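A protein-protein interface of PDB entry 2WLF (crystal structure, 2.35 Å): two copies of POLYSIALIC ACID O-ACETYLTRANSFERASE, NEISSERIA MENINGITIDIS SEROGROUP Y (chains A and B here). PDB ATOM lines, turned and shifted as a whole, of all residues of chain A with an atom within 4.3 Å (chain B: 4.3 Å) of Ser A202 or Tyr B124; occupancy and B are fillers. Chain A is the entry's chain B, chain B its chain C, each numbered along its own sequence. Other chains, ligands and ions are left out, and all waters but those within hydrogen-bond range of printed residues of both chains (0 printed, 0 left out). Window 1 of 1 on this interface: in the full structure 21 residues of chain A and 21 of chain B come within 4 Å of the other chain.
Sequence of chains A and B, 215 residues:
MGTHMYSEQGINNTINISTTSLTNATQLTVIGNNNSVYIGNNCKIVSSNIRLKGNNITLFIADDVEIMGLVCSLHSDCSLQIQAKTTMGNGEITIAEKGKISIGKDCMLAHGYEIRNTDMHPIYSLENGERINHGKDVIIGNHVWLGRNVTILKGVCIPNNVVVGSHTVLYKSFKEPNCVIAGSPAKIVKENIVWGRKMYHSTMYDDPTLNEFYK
The backbone carbonyl oxygen (O) of Asp A206 lies close to a ring nitrogen (NE2) of His A201 (3.1 Å). N of Thr A203 lies within hydrogen-bond range of OD1 of Asp A206. The backbone carbonyl oxygen of Glu B130 lies within hydrogen-bond range of the backbone NH of Ser B125 (2.7 Å).
Among the printed residues, pairs that only touch across the chains: Val A194 with Leu B126 (3.0 Å), Thr A203 with Gly B129 (3.2 Å), Lys A198 with Pro B122 (3.3 Å), Ile A193 with Tyr B124 (3.3 Å), Thr A203 with Tyr B124 (3.4 Å), Met A204 with Tyr B124 (3.5 Å), Lys A198 with Tyr B124 (3.5 Å), Ile A193 with Leu B126 (3.6 Å), Ser A202 with Tyr B124 (3.6 Å), Leu A210 with Tyr B124 (3.6 Å), Val A194 with Ile B123 (3.7 Å), Thr A203 with Glu B130 (3.7 Å), Ile A193 with Ile B123 (3.8 Å), Ser A202 with Arg B131 (3.8 Å) and Met A204 with Leu B126 (3.95 Å).
The backbone carbonyl oxygen (O) of Val A194 sits at hydrogen-bond distance from the backbone NH (N) of Tyr B124 (2.8 Å). The backbone carbonyl oxygen (O) of Pro B122 sits at hydrogen-bond distance from the backbone NH (N) of Gly A196 (3.0 Å). The side-chain hydroxyl of Tyr B124 is in hydrogen-bond range of the backbone carbonyl oxygen of His A201, at 3.0 Å. The backbone NH (N) of Met A204 is in hydrogen-bond range of the backbone carbonyl oxygen (O) of Gly B129, 3.1 Å away. The backbone carbonyl oxygen (O) of Ser B125 sits close to the side-chain sulfur (SD) of Met A204, at 3.8 Å.
Of the printed residues of chain B, Ser A202 touches Tyr B124 and Arg B131. Of the printed residues of chain A, Pro B122 touches Gly A196 (3.0 Å) and Lys A198 (3.3 Å). Of the printed residues of chain A, Tyr B124 touches Ile A193, Val A194, Lys A198, His A201, Ser A202, Thr A203, Met A204 and Leu A210. Of the printed residues of chain A, Ser B125 touches Met A204 (3.8 Å).
No position is printed for both chains.
Of the 11 printed residues of chain A, 9 touch a printed residue of chain B. Along chain A the printed residues that touch a printed residue of chain B span positions 193 to 210. Of the 8 printed residues of chain B, 8 touch a printed residue of chain A. Hydrophobic or aromatic side chains of chain B that line the printed part of chain A: Pro B122, Ile B123, Tyr B124 and Leu B126. Among the printed residues, 20 pairs touch across the chains.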
ATOM      1  N   ILE A 193     -21.781   4.810 -26.877  1.00  0.00           N
ATOM      2  CA  ILE A 193     -20.406   4.609 -26.452  1.00  0.00           C
ATOM      3  C   ILE A 193     -20.321   3.610 -25.305  1.00  0.00           C
ATOM      4  O   ILE A 193     -21.334   3.145 -24.776  1.00  0.00           O
ATOM      5  CB  ILE A 193     -19.771   5.947 -26.013  1.00  0.00           C
ATOM      6  CG1 ILE A 193     -20.573   6.596 -24.873  1.00  0.00           C
ATOM      7  CG2 ILE A 193     -19.703   6.901 -27.192  1.00  0.00           C
ATOM      8  CD1 ILE A 193     -20.424   5.905 -23.532  1.00  0.00           C
ATOM      9  N   VAL A 194     -19.099   3.270 -24.926  1.00  0.00           N
ATOM     10  CA  VAL A 194     -18.889   2.469 -23.739  1.00  0.00           C
ATOM     11  C   VAL A 194     -17.515   2.794 -23.197  1.00  0.00           C
ATOM     12  O   VAL A 194     -16.553   2.905 -23.955  1.00  0.00           O
ATOM     13  CB  VAL A 194     -19.024   0.954 -24.011  1.00  0.00           C
ATOM     14  CG1 VAL A 194     -18.278   0.556 -25.269  1.00  0.00           C
ATOM     15  CG2 VAL A 194     -18.528   0.145 -22.801  1.00  0.00           C
ATOM     16  N   GLY A 196     -14.185   2.300 -20.459  1.00  0.00           N
ATOM     17  CA  GLY A 196     -13.380   1.283 -19.792  1.00  0.00           C
ATOM     18  C   GLY A 196     -12.412   1.942 -18.833  1.00  0.00           C
ATOM     19  O   GLY A 196     -12.311   3.165 -18.784  1.00  0.00           O
ATOM     20  N   LYS A 198      -8.956   0.847 -18.366  1.00  0.00           N
ATOM     21  CA  LYS A 198      -7.571   0.797 -18.796  1.00  0.00           C
ATOM     22  C   LYS A 198      -7.397   1.404 -20.181  1.00  0.00           C
ATOM     23  O   LYS A 198      -8.017   0.957 -21.147  1.00  0.00           O
ATOM     24  CB  LYS A 198      -7.084  -0.650 -18.770  1.00  0.00           C
ATOM     25  CG  LYS A 198      -7.201  -1.296 -17.394  1.00  0.00           C
ATOM     26  N   TYR A 200      -4.625   1.428 -21.909  1.00  0.00           N
ATOM     27  CA  TYR A 200      -3.748   0.595 -22.705  1.00  0.00           C
ATOM     28  C   TYR A 200      -4.510  -0.444 -23.523  1.00  0.00           C
ATOM     29  O   TYR A 200      -3.898  -1.233 -24.234  1.00  0.00           O
ATOM     30  CB  TYR A 200      -2.690  -0.068 -21.822  1.00  0.00           C
ATOM     31  CG  TYR A 200      -3.221  -0.779 -20.593  1.00  0.00           C
ATOM     32  CD1 TYR A 200      -3.966  -1.947 -20.708  1.00  0.00           C
ATOM     33  CD2 TYR A 200      -2.942  -0.302 -19.313  1.00  0.00           C
ATOM     34  CE1 TYR A 200      -4.441  -2.610 -19.589  1.00  0.00           C
ATOM     35  CE2 TYR A 200      -3.410  -0.960 -18.183  1.00  0.00           C
ATOM     36  CZ  TYR A 200      -4.160  -2.115 -18.331  1.00  0.00           C
ATOM     37  OH  TYR A 200      -4.634  -2.778 -17.222  1.00  0.00           O
ATOM     38  N   HIS A 201      -5.837  -0.445 -23.431  1.00  0.00           N
ATOM     39  CA  HIS A 201      -6.661  -1.240 -24.344  1.00  0.00           C
ATOM     40  C   HIS A 201      -7.095  -0.378 -25.528  1.00  0.00           C
ATOM     41  O   HIS A 201      -7.835   0.607 -25.372  1.00  0.00           O
ATOM     42  CB  HIS A 201      -7.885  -1.829 -23.637  1.00  0.00           C
ATOM     43  CG  HIS A 201      -7.561  -2.949 -22.696  1.00  0.00           C
ATOM     44  ND1 HIS A 201      -7.723  -2.847 -21.331  1.00  0.00           N
ATOM     45  CD2 HIS A 201      -7.079  -4.193 -22.925  1.00  0.00           C
ATOM     46  CE1 HIS A 201      -7.358  -3.980 -20.759  1.00  0.00           C
ATOM     47  NE2 HIS A 201      -6.964  -4.813 -21.704  1.00  0.00           N
ATOM     48  N   SER A 202      -6.614  -0.751 -26.709  1.00  0.00           N
ATOM     49  CA  SER A 202      -6.835   0.016 -27.924  1.00  0.00           C
ATOM     50  C   SER A 202      -8.318   0.089 -28.239  1.00  0.00           C
ATOM     51  O   SER A 202      -8.828   1.127 -28.635  1.00  0.00           O
ATOM     52  CB  SER A 202      -6.116  -0.641 -29.108  1.00  0.00           C
ATOM     53  OG  SER A 202      -5.218  -1.660 -28.686  1.00  0.00           O
ATOM     54  N   THR A 203      -9.007  -1.033 -28.092  1.00  0.00           N
ATOM     55  CA  THR A 203     -10.413  -1.099 -28.444  1.00  0.00           C
ATOM     56  C   THR A 203     -11.159  -1.819 -27.355  1.00  0.00           C
ATOM     57  O   THR A 203     -10.560  -2.477 -26.516  1.00  0.00           O
ATOM     58  CB  THR A 203     -10.633  -1.881 -29.753  1.00  0.00           C
ATOM     59  OG1 THR A 203     -10.491  -3.283 -29.504  1.00  0.00           O
ATOM     60  CG2 THR A 203      -9.639  -1.444 -30.811  1.00  0.00           C
ATOM     61  N   MET A 204     -12.476  -1.717 -27.384  1.00  0.00           N
ATOM     62  CA  MET A 204     -13.279  -2.355 -26.367  1.00  0.00           C
ATOM     63  C   MET A 204     -13.051  -3.864 -26.369  1.00  0.00           C
ATOM     64  O   MET A 204     -12.991  -4.484 -25.306  1.00  0.00           O
ATOM     65  CB  MET A 204     -14.756  -2.010 -26.561  1.00  0.00           C
ATOM     66  CG  MET A 204     -15.405  -2.638 -27.764  1.00  0.00           C
ATOM     67  SD  MET A 204     -16.949  -1.789 -28.103  1.00  0.00           S
ATOM     68  CE  MET A 204     -17.760  -2.931 -29.222  1.00  0.00           C
ATOM     69  N   ASP A 206     -10.588  -5.547 -26.617  1.00  0.00           N
ATOM     70  CA  ASP A 206      -9.366  -5.929 -25.931  1.00  0.00           C
ATOM     71  C   ASP A 206      -9.622  -5.928 -24.433  1.00  0.00           C
ATOM     72  O   ASP A 206      -8.770  -6.341 -23.645  1.00  0.00           O
ATOM     73  CB  ASP A 206      -8.243  -4.948 -26.266  1.00  0.00           C
ATOM     74  CG  ASP A 206      -8.113  -4.695 -27.761  1.00  0.00           C
ATOM     75  OD1 ASP A 206      -8.558  -3.620 -28.238  1.00  0.00           O
ATOM     76  OD2 ASP A 206      -7.570  -5.572 -28.455  1.00  0.00           O
ATOM     77  N   LEU A 210     -15.788  -5.769 -20.873  1.00  0.00           N
ATOM     78  CA  LEU A 210     -16.707  -4.974 -21.687  1.00  0.00           C
ATOM     79  C   LEU A 210     -17.537  -5.844 -22.627  1.00  0.00           C
ATOM     80  O   LEU A 210     -18.410  -5.351 -23.336  1.00  0.00           O
ATOM     81  CB  LEU A 210     -15.933  -3.926 -22.493  1.00  0.00           C
ATOM     82  CG  LEU A 210     -15.140  -2.915 -21.662  1.00  0.00           C
ATOM     83  CD1 LEU A 210     -14.277  -2.016 -22.539  1.00  0.00           C
ATOM     84  CD2 LEU A 210     -16.083  -2.085 -20.811  1.00  0.00           C
ATOM     85  N   PRO B 122     -10.450   5.336 -21.204  1.00  0.00           N
ATOM     86  CA  PRO B 122     -10.869   5.356 -22.587  1.00  0.00           C
ATOM     87  C   PRO B 122     -12.367   5.287 -22.729  1.00  0.00           C
ATOM     88  O   PRO B 122     -13.038   4.639 -21.921  1.00  0.00           O
ATOM     89  CB  PRO B 122     -10.253   4.082 -23.148  1.00  0.00           C
ATOM     90  CG  PRO B 122     -10.315   3.127 -22.004  1.00  0.00           C
ATOM     91  CD  PRO B 122     -10.121   3.973 -20.755  1.00  0.00           C
ATOM     92  N   ILE B 123     -12.878   5.978 -23.742  1.00  0.00           N
ATOM     93  CA  ILE B 123     -14.255   5.836 -24.168  1.00  0.00           C
ATOM     94  C   ILE B 123     -14.221   5.287 -25.585  1.00  0.00           C
ATOM     95  O   ILE B 123     -13.524   5.828 -26.445  1.00  0.00           O
ATOM     96  CB  ILE B 123     -14.991   7.175 -24.160  1.00  0.00           C
ATOM     97  CG1 ILE B 123     -15.171   7.662 -22.722  1.00  0.00           C
ATOM     98  CG2 ILE B 123     -16.342   7.023 -24.804  1.00  0.00           C
ATOM     99  CD1 ILE B 123     -15.808   9.012 -22.616  1.00  0.00           C
ATOM    100  N   TYR B 124     -14.950   4.205 -25.828  1.00  0.00           N
ATOM    101  CA  TYR B 124     -14.932   3.575 -27.142  1.00  0.00           C
ATOM    102  C   TYR B 124     -16.266   3.737 -27.832  1.00  0.00           C
ATOM    103  O   TYR B 124     -17.311   3.801 -27.179  1.00  0.00           O
ATOM    104  CB  TYR B 124     -14.655   2.083 -27.035  1.00  0.00           C
ATOM    105  CG  TYR B 124     -13.502   1.683 -26.155  1.00  0.00           C
ATOM    106  CD1 TYR B 124     -12.214   1.648 -26.643  1.00  0.00           C
ATOM    107  CD2 TYR B 124     -13.717   1.285 -24.848  1.00  0.00           C
ATOM    108  CE1 TYR B 124     -11.154   1.246 -25.843  1.00  0.00           C
ATOM    109  CE2 TYR B 124     -12.665   0.883 -24.034  1.00  0.00           C
ATOM    110  CZ  TYR B 124     -11.393   0.866 -24.540  1.00  0.00           C
ATOM    111  OH  TYR B 124     -10.358   0.466 -23.736  1.00  0.00           O
ATOM    112  N   SER B 125     -16.226   3.780 -29.157  1.00  0.00           N
ATOM    113  CA  SER B 125     -17.440   3.743 -29.957  1.00  0.00           C
ATOM    114  C   SER B 125     -18.017   2.337 -29.937  1.00  0.00           C
ATOM    115  O   SER B 125     -17.305   1.367 -30.135  1.00  0.00           O
ATOM    116  CB  SER B 125     -17.149   4.138 -31.399  1.00  0.00           C
ATOM    117  OG  SER B 125     -18.327   4.039 -32.175  1.00  0.00           O
ATOM    118  N   LEU B 126     -19.312   2.238 -29.678  1.00  0.00           N
ATOM    119  CA  LEU B 126     -19.998   0.962 -29.701  1.00  0.00           C
ATOM    120  C   LEU B 126     -20.097   0.515 -31.153  1.00  0.00           C
ATOM    121  O   LEU B 126     -20.256  -0.664 -31.449  1.00  0.00           O
ATOM    122  CB  LEU B 126     -21.390   1.120 -29.089  1.00  0.00           C
ATOM    123  CG  LEU B 126     -21.709   0.164 -27.939  1.00  0.00           C
ATOM    124  CD1 LEU B 126     -20.441  -0.184 -27.173  1.00  0.00           C
ATOM    125  CD2 LEU B 126     -22.757   0.759 -27.005  1.00  0.00           C
ATOM    126  N   GLY B 129     -15.845  -0.015 -31.875  1.00  0.00           N
ATOM    127  CA  GLY B 129     -14.965  -0.398 -30.769  1.00  0.00           C
ATOM    128  C   GLY B 129     -13.757   0.508 -30.632  1.00  0.00           C
ATOM    129  O   GLY B 129     -12.914   0.324 -29.741  1.00  0.00           O
ATOM    130  N   GLU B 130     -13.666   1.492 -31.516  1.00  0.00           N
ATOM    131  CA  GLU B 130     -12.524   2.387 -31.506  1.00  0.00           C
ATOM    132  C   GLU B 130     -12.607   3.381 -30.346  1.00  0.00           C
ATOM    133  O   GLU B 130     -13.689   3.781 -29.924  1.00  0.00           O
ATOM    134  CB  GLU B 130     -12.410   3.116 -32.846  1.00  0.00           C
ATOM    135  CG  GLU B 130     -12.201   2.169 -34.043  1.00  0.00           C
ATOM    136  CD  GLU B 130     -11.130   1.109 -33.786  1.00  0.00           C
ATOM    137  OE1 GLU B 130      -9.954   1.483 -33.589  1.00  0.00           O
ATOM    138  OE2 GLU B 130     -11.465  -0.102 -33.787  1.00  0.00           O
ATOM    139  N   ARG B 131     -11.446   3.744 -29.816  1.00  0.00           N
ATOM    140  CA  ARG B 131     -11.358   4.781 -28.802  1.00  0.00           C
ATOM    141  C   ARG B 131     -11.552   6.155 -29.435  1.00  0.00           C
ATOM    142  O   ARG B 131     -10.966   6.457 -30.477  1.00  0.00           O
ATOM    143  CB  ARG B 131     -10.008   4.741 -28.092  1.00  0.00           C
ATOM    144  CG  ARG B 131      -9.995   5.677 -26.921  1.00  0.00           C
ATOM    145  CD  ARG B 131      -8.675   5.756 -26.178  1.00  0.00           C
ATOM    146  NE  ARG B 131      -8.748   6.862 -25.227  1.00  0.00           N
ATOM    147  CZ  ARG B 131      -7.714   7.369 -24.575  1.00  0.00           C
ATOM    148  NH1 ARG B 131      -6.503   6.870 -24.748  1.00  0.00           N
ATOM    149  NH2 ARG B 131      -7.897   8.387 -23.754  1.00  0.00           N
